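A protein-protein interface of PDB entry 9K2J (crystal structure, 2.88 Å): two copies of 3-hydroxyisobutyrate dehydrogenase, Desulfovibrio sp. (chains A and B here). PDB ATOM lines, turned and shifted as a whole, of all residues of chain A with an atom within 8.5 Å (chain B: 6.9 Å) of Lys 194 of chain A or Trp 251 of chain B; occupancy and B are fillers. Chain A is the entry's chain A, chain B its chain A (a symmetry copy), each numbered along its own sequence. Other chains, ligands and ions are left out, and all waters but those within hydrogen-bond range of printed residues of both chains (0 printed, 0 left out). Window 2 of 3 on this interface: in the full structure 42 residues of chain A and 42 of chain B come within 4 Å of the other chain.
No position is printed for both chains.
Of the 10 pairs that touch across the chains among the printed residues, none has its exchanged pair printed and touching as well.
Of the 15 printed residues of chain A, 7 touch a printed residue of chain B.
Printed residues of chain A that touch a printed residue of chain B: Gly 188, Arg 190, Ile 191, Gly 192, Lys 194, Ala 195 and Ile 197.
Hydrophobic or aromatic side chains of chain A within 4 Å of the printed part of chain B: Ile 191, Ala 195 and Ile 197.
Of the 15 printed residues of chain B, 6 touch a printed residue of chain A.
Hydrophobic or aromatic side chains of chain B within 4 Å of the printed part of chain A: Ala 166, Ala 169, Ile 173, Met 247, Trp 251 and Met 253.
Among the printed residues, 10 pairs touch across the chains.
Among the printed residues, no Asp or Glu carboxylate lies within 4 Å of a Lys or Arg side-chain nitrogen of the other chain.
Among the printed residues, merely in contact across the chains: Gly 192 of chain A with Ile 173 of chain B, Ala 195 of chain A with Ala 169 of chain B, Arg 190 of chain A with Met 253 of chain B, Ile 191 of chain A with Ile 173 of chain B, Ala 195 of chain A with Trp 251 of chain B, Gly 188 of chain A with Ile 173 of chain B, Ile 191 of chain A with Met 253 of chain B, Ile 197 of chain A with Ala 166 of chain B, Lys 194 of chain A with Trp 251 of chain B and Ile 191 of chain A with Met 247 of chain B.
Lys 194 of chain A touches one residue of chain B.
Trp 251 of chain B touches two residues of chain A.
No residue of chain A comes within 4 Å of Ala 250 of chain B.
Gly 252 of chain B touches none of the printed residues of chain A.
Printed residues of chain A within 4 Å of Met 247 of chain B: Ile 191 (3.99 Å).
Of the printed residues of chain B, Gly 192 of chain A touches Ile 173 (3.4 Å).
Of the printed residues of chain A, Ala 166 of chain B touches Ile 197 (3.8 Å).
Of the printed residues of chain B, Gly 188 of chain A touches Ile 173 (3.7 Å).
Printed residues of chain A within 4 Å of Ala 169 of chain B: Ala 195.
Glu 246 of chain B touches none of the printed residues of chain A.
The nearest residue of chain A that does not touch Trp 251 of chain B is Ile 191 of chain A (4.2 Å).
The guanidinium group (NH2) of Arg 190 of chain A lies within salt-bridge range of the side-chain carboxylate (OE1) of Glu 193 of chain A.
N of Ile 197 of chain A is in hydrogen-bond range of O of Gly 192 of chain A, 2.9 Å away.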
ATOM      1  N   GLU A 187     -20.248 -16.355   4.429  1.00  0.00           N
ATOM      2  CA  GLU A 187     -20.360 -15.552   3.215  1.00  0.00           C
ATOM      3  C   GLU A 187     -19.062 -15.603   2.407  1.00  0.00           C
ATOM      4  O   GLU A 187     -19.084 -15.806   1.186  1.00  0.00           O
ATOM      5  CB  GLU A 187     -20.737 -14.113   3.574  1.00  0.00           C
ATOM      6  CG  GLU A 187     -22.209 -13.961   3.993  1.00  0.00           C
ATOM      7  CD  GLU A 187     -22.653 -12.504   4.284  1.00  0.00           C
ATOM      8  OE1 GLU A 187     -21.838 -11.561   4.157  1.00  0.00           O
ATOM      9  OE2 GLU A 187     -23.847 -12.296   4.609  1.00  0.00           O
ATOM     10  N   GLY A 188     -17.917 -15.482   3.084  1.00  0.00           N
ATOM     11  CA  GLY A 188     -16.645 -15.538   2.378  1.00  0.00           C
ATOM     12  C   GLY A 188     -16.402 -16.875   1.697  1.00  0.00           C
ATOM     13  O   GLY A 188     -15.927 -16.924   0.556  1.00  0.00           O
ATOM     14  N   ILE A 189     -16.697 -17.978   2.400  1.00  0.00           N
ATOM     15  CA  ILE A 189     -16.470 -19.322   1.865  1.00  0.00           C
ATOM     16  C   ILE A 189     -17.360 -19.557   0.655  1.00  0.00           C
ATOM     17  O   ILE A 189     -16.935 -20.115  -0.369  1.00  0.00           O
ATOM     18  CB  ILE A 189     -16.735 -20.373   2.960  1.00  0.00           C
ATOM     19  CG1 ILE A 189     -15.571 -20.463   3.932  1.00  0.00           C
ATOM     20  CG2 ILE A 189     -16.999 -21.744   2.346  1.00  0.00           C
ATOM     21  CD1 ILE A 189     -15.840 -21.400   5.042  1.00  0.00           C
ATOM     22  N   ARG A 190     -18.605 -19.099   0.745  1.00  0.00           N
ATOM     23  CA  ARG A 190     -19.559 -19.274  -0.341  1.00  0.00           C
ATOM     24  C   ARG A 190     -19.179 -18.431  -1.562  1.00  0.00           C
ATOM     25  O   ARG A 190     -19.300 -18.886  -2.717  1.00  0.00           O
ATOM     26  CB  ARG A 190     -20.944 -18.907   0.181  1.00  0.00           C
ATOM     27  CG  ARG A 190     -21.981 -18.798  -0.895  1.00  0.00           C
ATOM     28  CD  ARG A 190     -22.705 -20.050  -1.515  1.00  0.00           C
ATOM     29  NE  ARG A 190     -21.891 -20.838  -2.432  1.00  0.00           N
ATOM     30  CZ  ARG A 190     -22.353 -21.859  -3.177  1.00  0.00           C
ATOM     31  NH1 ARG A 190     -23.684 -22.058  -3.360  1.00  0.00           N
ATOM     32  NH2 ARG A 190     -21.498 -22.567  -3.917  1.00  0.00           N
ATOM     33  N   ILE A 191     -18.652 -17.225  -1.327  1.00  0.00           N
ATOM     34  CA  ILE A 191     -18.107 -16.430  -2.430  1.00  0.00           C
ATOM     35  C   ILE A 191     -16.962 -17.171  -3.095  1.00  0.00           C
ATOM     36  O   ILE A 191     -16.901 -17.284  -4.323  1.00  0.00           O
ATOM     37  CB  ILE A 191     -17.631 -15.052  -1.941  1.00  0.00           C
ATOM     38  CG1 ILE A 191     -18.787 -14.177  -1.491  1.00  0.00           C
ATOM     39  CG2 ILE A 191     -16.854 -14.333  -3.048  1.00  0.00           C
ATOM     40  CD1 ILE A 191     -18.300 -12.955  -0.765  1.00  0.00           C
ATOM     41  N   GLY A 192     -16.030 -17.678  -2.291  1.00  0.00           N
ATOM     42  CA  GLY A 192     -14.918 -18.423  -2.849  1.00  0.00           C
ATOM     43  C   GLY A 192     -15.374 -19.594  -3.690  1.00  0.00           C
ATOM     44  O   GLY A 192     -14.746 -19.925  -4.697  1.00  0.00           O
ATOM     45  N   GLU A 193     -16.485 -20.220  -3.309  1.00  0.00           N
ATOM     46  CA  GLU A 193     -17.006 -21.314  -4.127  1.00  0.00           C
ATOM     47  C   GLU A 193     -17.531 -20.821  -5.478  1.00  0.00           C
ATOM     48  O   GLU A 193     -17.347 -21.490  -6.506  1.00  0.00           O
ATOM     49  CB  GLU A 193     -18.107 -22.050  -3.371  1.00  0.00           C
ATOM     50  CG  GLU A 193     -17.616 -22.767  -2.152  1.00  0.00           C
ATOM     51  CD  GLU A 193     -18.612 -23.785  -1.673  1.00  0.00           C
ATOM     52  OE1 GLU A 193     -19.813 -23.426  -1.617  1.00  0.00           O
ATOM     53  OE2 GLU A 193     -18.187 -24.933  -1.374  1.00  0.00           O
ATOM     54  N   LYS A 194     -18.165 -19.647  -5.511  1.00  0.00           N
ATOM     55  CA  LYS A 194     -18.558 -19.105  -6.815  1.00  0.00           C
ATOM     56  C   LYS A 194     -17.363 -18.728  -7.704  1.00  0.00           C
ATOM     57  O   LYS A 194     -17.524 -18.595  -8.923  1.00  0.00           O
ATOM     58  CB  LYS A 194     -19.494 -17.921  -6.612  1.00  0.00           C
ATOM     59  CG  LYS A 194     -20.762 -18.360  -5.908  1.00  0.00           C
ATOM     60  CD  LYS A 194     -21.784 -18.736  -6.934  1.00  0.00           C
ATOM     61  CE  LYS A 194     -23.120 -19.075  -6.350  1.00  0.00           C
ATOM     62  NZ  LYS A 194     -24.083 -18.983  -7.479  1.00  0.00           N
ATOM     63  N   ALA A 195     -16.180 -18.548  -7.131  1.00  0.00           N
ATOM     64  CA  ALA A 195     -14.974 -18.331  -7.910  1.00  0.00           C
ATOM     65  C   ALA A 195     -14.242 -19.628  -8.230  1.00  0.00           C
ATOM     66  O   ALA A 195     -13.153 -19.576  -8.818  1.00  0.00           O
ATOM     67  CB  ALA A 195     -14.030 -17.385  -7.167  1.00  0.00           C
ATOM     68  N   GLY A 196     -14.799 -20.776  -7.835  1.00  0.00           N
ATOM     69  CA  GLY A 196     -14.166 -22.056  -8.091  1.00  0.00           C
ATOM     70  C   GLY A 196     -13.006 -22.398  -7.185  1.00  0.00           C
ATOM     71  O   GLY A 196     -12.125 -23.169  -7.579  1.00  0.00           O
ATOM     72  N   ILE A 197     -12.983 -21.853  -5.975  1.00  0.00           N
ATOM     73  CA  ILE A 197     -11.963 -22.160  -4.980  1.00  0.00           C
ATOM     74  C   ILE A 197     -12.568 -23.159  -4.009  1.00  0.00           C
ATOM     75  O   ILE A 197     -13.641 -22.917  -3.439  1.00  0.00           O
ATOM     76  CB  ILE A 197     -11.489 -20.890  -4.248  1.00  0.00           C
ATOM     77  CG1 ILE A 197     -11.144 -19.790  -5.247  1.00  0.00           C
ATOM     78  CG2 ILE A 197     -10.316 -21.185  -3.337  1.00  0.00           C
ATOM     79  CD1 ILE A 197     -10.974 -18.472  -4.621  1.00  0.00           C
ATOM     80  N   LYS A 198     -11.906 -24.294  -3.837  1.00  0.00           N
ATOM     81  CA  LYS A 198     -12.362 -25.252  -2.844  1.00  0.00           C
ATOM     82  C   LYS A 198     -12.253 -24.649  -1.445  1.00  0.00           C
ATOM     83  O   LYS A 198     -11.284 -23.957  -1.124  1.00  0.00           O
ATOM     84  CB  LYS A 198     -11.557 -26.546  -2.960  1.00  0.00           C
ATOM     85  CG  LYS A 198     -12.234 -27.729  -2.292  1.00  0.00           C
ATOM     86  CD  LYS A 198     -11.459 -29.036  -2.409  1.00  0.00           C
ATOM     87  CE  LYS A 198     -12.255 -30.149  -1.747  1.00  0.00           C
ATOM     88  NZ  LYS A 198     -12.088 -30.058  -0.267  1.00  0.00           N
ATOM     89  N   LEU A 202      -9.344 -22.211   0.290  1.00  0.00           N
ATOM     90  CA  LEU A 202      -9.672 -20.856   0.693  1.00  0.00           C
ATOM     91  C   LEU A 202      -9.334 -20.640   2.162  1.00  0.00           C
ATOM     92  O   LEU A 202      -8.700 -19.638   2.505  1.00  0.00           O
ATOM     93  CB  LEU A 202     -11.139 -20.552   0.442  1.00  0.00           C
ATOM     94  CG  LEU A 202     -11.406 -19.058   0.704  1.00  0.00           C
ATOM     95  CD1 LEU A 202     -10.893 -18.146  -0.410  1.00  0.00           C
ATOM     96  CD2 LEU A 202     -12.894 -18.786   0.985  1.00  0.00           C
ATOM     97  N   THR A 285     -26.532 -19.918   3.168  1.00  0.00           N
ATOM     98  CA  THR A 285     -25.857 -18.666   2.825  1.00  0.00           C
ATOM     99  C   THR A 285     -25.744 -18.509   1.314  1.00  0.00           C
ATOM    100  O   THR A 285     -25.208 -19.389   0.628  1.00  0.00           O
ATOM    101  CB  THR A 285     -24.454 -18.626   3.428  1.00  0.00           C
ATOM    102  OG1 THR A 285     -24.536 -18.567   4.857  1.00  0.00           O
ATOM    103  CG2 THR A 285     -23.689 -17.427   2.916  1.00  0.00           C
ATOM    104  N   GLU A 286     -26.170 -17.363   0.797  1.00  0.00           N
ATOM    105  CA  GLU A 286     -26.092 -17.206  -0.649  1.00  0.00           C
ATOM    106  C   GLU A 286     -25.921 -15.758  -1.133  1.00  0.00           C
ATOM    107  O   GLU A 286     -25.548 -14.874  -0.369  1.00  0.00           O
ATOM    108  CB  GLU A 286     -27.354 -17.813  -1.283  1.00  0.00           C
ATOM    109  CG  GLU A 286     -28.583 -16.932  -1.125  1.00  0.00           C
ATOM    110  CD  GLU A 286     -29.890 -17.681  -1.267  1.00  0.00           C
ATOM    111  OE1 GLU A 286     -30.899 -17.020  -1.626  1.00  0.00           O
ATOM    112  OE2 GLU A 286     -29.911 -18.916  -1.012  1.00  0.00           O
ATOM    113  N   PRO B  99     -12.934 -10.050 -10.984  1.00  0.00           N
ATOM    114  CA  PRO B  99     -12.692 -11.137 -11.947  1.00  0.00           C
ATOM    115  C   PRO B  99     -13.158 -10.822 -13.354  1.00  0.00           C
ATOM    116  O   PRO B  99     -12.481 -11.198 -14.325  1.00  0.00           O
ATOM    117  CB  PRO B  99     -13.483 -12.310 -11.344  1.00  0.00           C
ATOM    118  CG  PRO B  99     -13.556 -11.994  -9.907  1.00  0.00           C
ATOM    119  CD  PRO B  99     -13.780 -10.510  -9.878  1.00  0.00           C
ATOM    120  N   GLN B 100     -14.282 -10.122 -13.495  1.00  0.00           N
ATOM    121  CA  GLN B 100     -14.744  -9.753 -14.830  1.00  0.00           C
ATOM    122  C   GLN B 100     -13.640  -9.036 -15.605  1.00  0.00           C
ATOM    123  O   GLN B 100     -13.316  -9.391 -16.755  1.00  0.00           O
ATOM    124  CB  GLN B 100     -15.978  -8.865 -14.708  1.00  0.00           C
ATOM    125  CG  GLN B 100     -17.026  -9.066 -15.772  1.00  0.00           C
ATOM    126  CD  GLN B 100     -18.277  -8.253 -15.485  1.00  0.00           C
ATOM    127  OE1 GLN B 100     -18.340  -7.054 -15.788  1.00  0.00           O
ATOM    128  NE2 GLN B 100     -19.272  -8.895 -14.876  1.00  0.00           N
ATOM    129  N   GLU B 165      -9.752 -15.769 -12.068  1.00  0.00           N
ATOM    130  CA  GLU B 165     -10.827 -15.236 -11.244  1.00  0.00           C
ATOM    131  C   GLU B 165     -10.615 -15.643  -9.789  1.00  0.00           C
ATOM    132  O   GLU B 165     -10.949 -14.884  -8.871  1.00  0.00           O
ATOM    133  CB  GLU B 165     -12.222 -15.615 -11.794  1.00  0.00           C
ATOM    134  CG  GLU B 165     -12.193 -15.361 -13.293  1.00  0.00           C
ATOM    135  CD  GLU B 165     -12.459 -16.589 -14.168  1.00  0.00           C
ATOM    136  OE1 GLU B 165     -13.258 -17.394 -13.704  1.00  0.00           O
ATOM    137  OE2 GLU B 165     -11.664 -16.933 -15.096  1.00  0.00           O
ATOM    138  N   ALA B 166     -10.033 -16.827  -9.562  1.00  0.00           N
ATOM    139  CA  ALA B 166      -9.646 -17.219  -8.212  1.00  0.00           C
ATOM    140  C   ALA B 166      -8.634 -16.243  -7.632  1.00  0.00           C
ATOM    141  O   ALA B 166      -8.729 -15.864  -6.456  1.00  0.00           O
ATOM    142  CB  ALA B 166      -9.071 -18.634  -8.229  1.00  0.00           C
ATOM    143  N   ALA B 169     -10.362 -13.222  -6.580  1.00  0.00           N
ATOM    144  CA  ALA B 169     -11.374 -13.458  -5.565  1.00  0.00           C
ATOM    145  C   ALA B 169     -10.757 -13.669  -4.201  1.00  0.00           C
ATOM    146  O   ALA B 169     -11.299 -13.210  -3.202  1.00  0.00           O
ATOM    147  CB  ALA B 169     -12.237 -14.654  -5.954  1.00  0.00           C
ATOM    148  N   ILE B 173     -11.903 -11.401  -1.189  1.00  0.00           N
ATOM    149  CA  ILE B 173     -12.571 -12.054  -0.064  1.00  0.00           C
ATOM    150  C   ILE B 173     -11.825 -11.755   1.222  1.00  0.00           C
ATOM    151  O   ILE B 173     -12.441 -11.514   2.268  1.00  0.00           O
ATOM    152  CB  ILE B 173     -12.697 -13.577  -0.296  1.00  0.00           C
ATOM    153  CG1 ILE B 173     -13.779 -13.896  -1.316  1.00  0.00           C
ATOM    154  CG2 ILE B 173     -13.027 -14.316   0.999  1.00  0.00           C
ATOM    155  CD1 ILE B 173     -13.654 -15.280  -1.887  1.00  0.00           C
ATOM    156  N   GLY B 244     -15.391  -5.985  -4.249  1.00  0.00           N
ATOM    157  CA  GLY B 244     -15.758  -7.367  -3.984  1.00  0.00           C
ATOM    158  C   GLY B 244     -17.261  -7.567  -3.946  1.00  0.00           C
ATOM    159  O   GLY B 244     -17.778  -8.583  -4.426  1.00  0.00           O
ATOM    160  N   GLU B 246     -19.463  -5.825  -5.626  1.00  0.00           N
ATOM    161  CA  GLU B 246     -19.875  -5.828  -7.031  1.00  0.00           C
ATOM    162  C   GLU B 246     -19.539  -7.158  -7.710  1.00  0.00           C
ATOM    163  O   GLU B 246     -20.313  -7.646  -8.554  1.00  0.00           O
ATOM    164  CB  GLU B 246     -19.199  -4.674  -7.775  1.00  0.00           C
ATOM    165  CG  GLU B 246     -19.848  -3.295  -7.615  1.00  0.00           C
ATOM    166  CD  GLU B 246     -18.924  -2.126  -8.048  1.00  0.00           C
ATOM    167  OE1 GLU B 246     -17.945  -2.350  -8.821  1.00  0.00           O
ATOM    168  OE2 GLU B 246     -19.189  -0.978  -7.601  1.00  0.00           O
ATOM    169  N   MET B 247     -18.387  -7.752  -7.345  1.00  0.00           N
ATOM    170  CA  MET B 247     -17.953  -9.026  -7.915  1.00  0.00           C
ATOM    171  C   MET B 247     -18.939 -10.140  -7.594  1.00  0.00           C
ATOM    172  O   MET B 247     -19.430 -10.830  -8.500  1.00  0.00           O
ATOM    173  CB  MET B 247     -16.566  -9.386  -7.390  1.00  0.00           C
ATOM    174  CG  MET B 247     -16.251 -10.846  -7.585  1.00  0.00           C
ATOM    175  SD  MET B 247     -14.860 -11.448  -6.620  1.00  0.00           S
ATOM    176  CE  MET B 247     -15.417 -11.137  -4.950  1.00  0.00           C
ATOM    177  N   ALA B 248     -19.250 -10.322  -6.303  1.00  0.00           N
ATOM    178  CA  ALA B 248     -20.453 -11.060  -5.937  1.00  0.00           C
ATOM    179  C   ALA B 248     -21.577 -10.164  -6.396  1.00  0.00           C
ATOM    180  O   ALA B 248     -21.310  -9.026  -6.729  1.00  0.00           O
ATOM    181  CB  ALA B 248     -20.506 -11.309  -4.440  1.00  0.00           C
ATOM    182  N   GLU B 249     -22.809 -10.645  -6.473  1.00  0.00           N
ATOM    183  CA  GLU B 249     -23.833  -9.752  -7.048  1.00  0.00           C
ATOM    184  C   GLU B 249     -23.745  -9.833  -8.568  1.00  0.00           C
ATOM    185  O   GLU B 249     -24.764 -10.078  -9.218  1.00  0.00           O
ATOM    186  CB  GLU B 249     -23.705  -8.274  -6.578  1.00  0.00           C
ATOM    187  CG  GLU B 249     -24.787  -7.249  -6.916  1.00  0.00           C
ATOM    188  CD  GLU B 249     -24.213  -5.797  -7.066  1.00  0.00           C
ATOM    189  OE1 GLU B 249     -24.474  -4.922  -6.199  1.00  0.00           O
ATOM    190  OE2 GLU B 249     -23.491  -5.526  -8.078  1.00  0.00           O
ATOM    191  N   ALA B 250     -22.549  -9.659  -9.155  1.00  0.00           N
ATOM    192  CA  ALA B 250     -22.390 -10.087 -10.547  1.00  0.00           C
ATOM    193  C   ALA B 250     -22.548 -11.597 -10.667  1.00  0.00           C
ATOM    194  O   ALA B 250     -22.911 -12.108 -11.734  1.00  0.00           O
ATOM    195  CB  ALA B 250     -21.028  -9.667 -11.100  1.00  0.00           C
ATOM    196  N   TRP B 251     -22.258 -12.319  -9.589  1.00  0.00           N
ATOM    197  CA  TRP B 251     -22.480 -13.745  -9.509  1.00  0.00           C
ATOM    198  C   TRP B 251     -23.852 -14.072  -8.933  1.00  0.00           C
ATOM    199  O   TRP B 251     -24.098 -15.216  -8.541  1.00  0.00           O
ATOM    200  CB  TRP B 251     -21.389 -14.401  -8.665  1.00  0.00           C
ATOM    201  CG  TRP B 251     -20.065 -14.614  -9.367  1.00  0.00           C
ATOM    202  CD1 TRP B 251     -19.871 -14.951 -10.671  1.00  0.00           C
ATOM    203  CD2 TRP B 251     -18.757 -14.561  -8.767  1.00  0.00           C
ATOM    204  NE1 TRP B 251     -18.522 -15.089 -10.931  1.00  0.00           N
ATOM    205  CE2 TRP B 251     -17.819 -14.847  -9.780  1.00  0.00           C
ATOM    206  CE3 TRP B 251     -18.290 -14.287  -7.470  1.00  0.00           C
ATOM    207  CZ2 TRP B 251     -16.436 -14.867  -9.541  1.00  0.00           C
ATOM    208  CZ3 TRP B 251     -16.911 -14.307  -7.234  1.00  0.00           C
ATOM    209  CH2 TRP B 251     -16.002 -14.597  -8.264  1.00  0.00           C
ATOM    210  N   GLY B 252     -24.730 -13.080  -8.822  1.00  0.00           N
ATOM    211  CA  GLY B 252     -26.048 -13.334  -8.287  1.00  0.00           C
ATOM    212  C   GLY B 252     -26.129 -13.474  -6.787  1.00  0.00           C
ATOM    213  O   GLY B 252     -27.101 -14.046  -6.295  1.00  0.00           O
ATOM    214  N   MET B 253     -25.149 -12.973  -6.035  1.00  0.00           N
ATOM    215  CA  MET B 253     -25.135 -13.246  -4.605  1.00  0.00           C
ATOM    216  C   MET B 253     -25.822 -12.146  -3.794  1.00  0.00           C
ATOM    217  O   MET B 253     -26.146 -11.076  -4.303  1.00  0.00           O
ATOM    218  CB  MET B 253     -23.708 -13.438  -4.110  1.00  0.00           C
ATOM    219  CG  MET B 253     -23.009 -14.543  -4.811  1.00  0.00           C
ATOM    220  SD  MET B 253     -21.449 -14.888  -4.001  1.00  0.00           S
ATOM    221  CE  MET B 253     -22.035 -15.697  -2.500  1.00  0.00           C
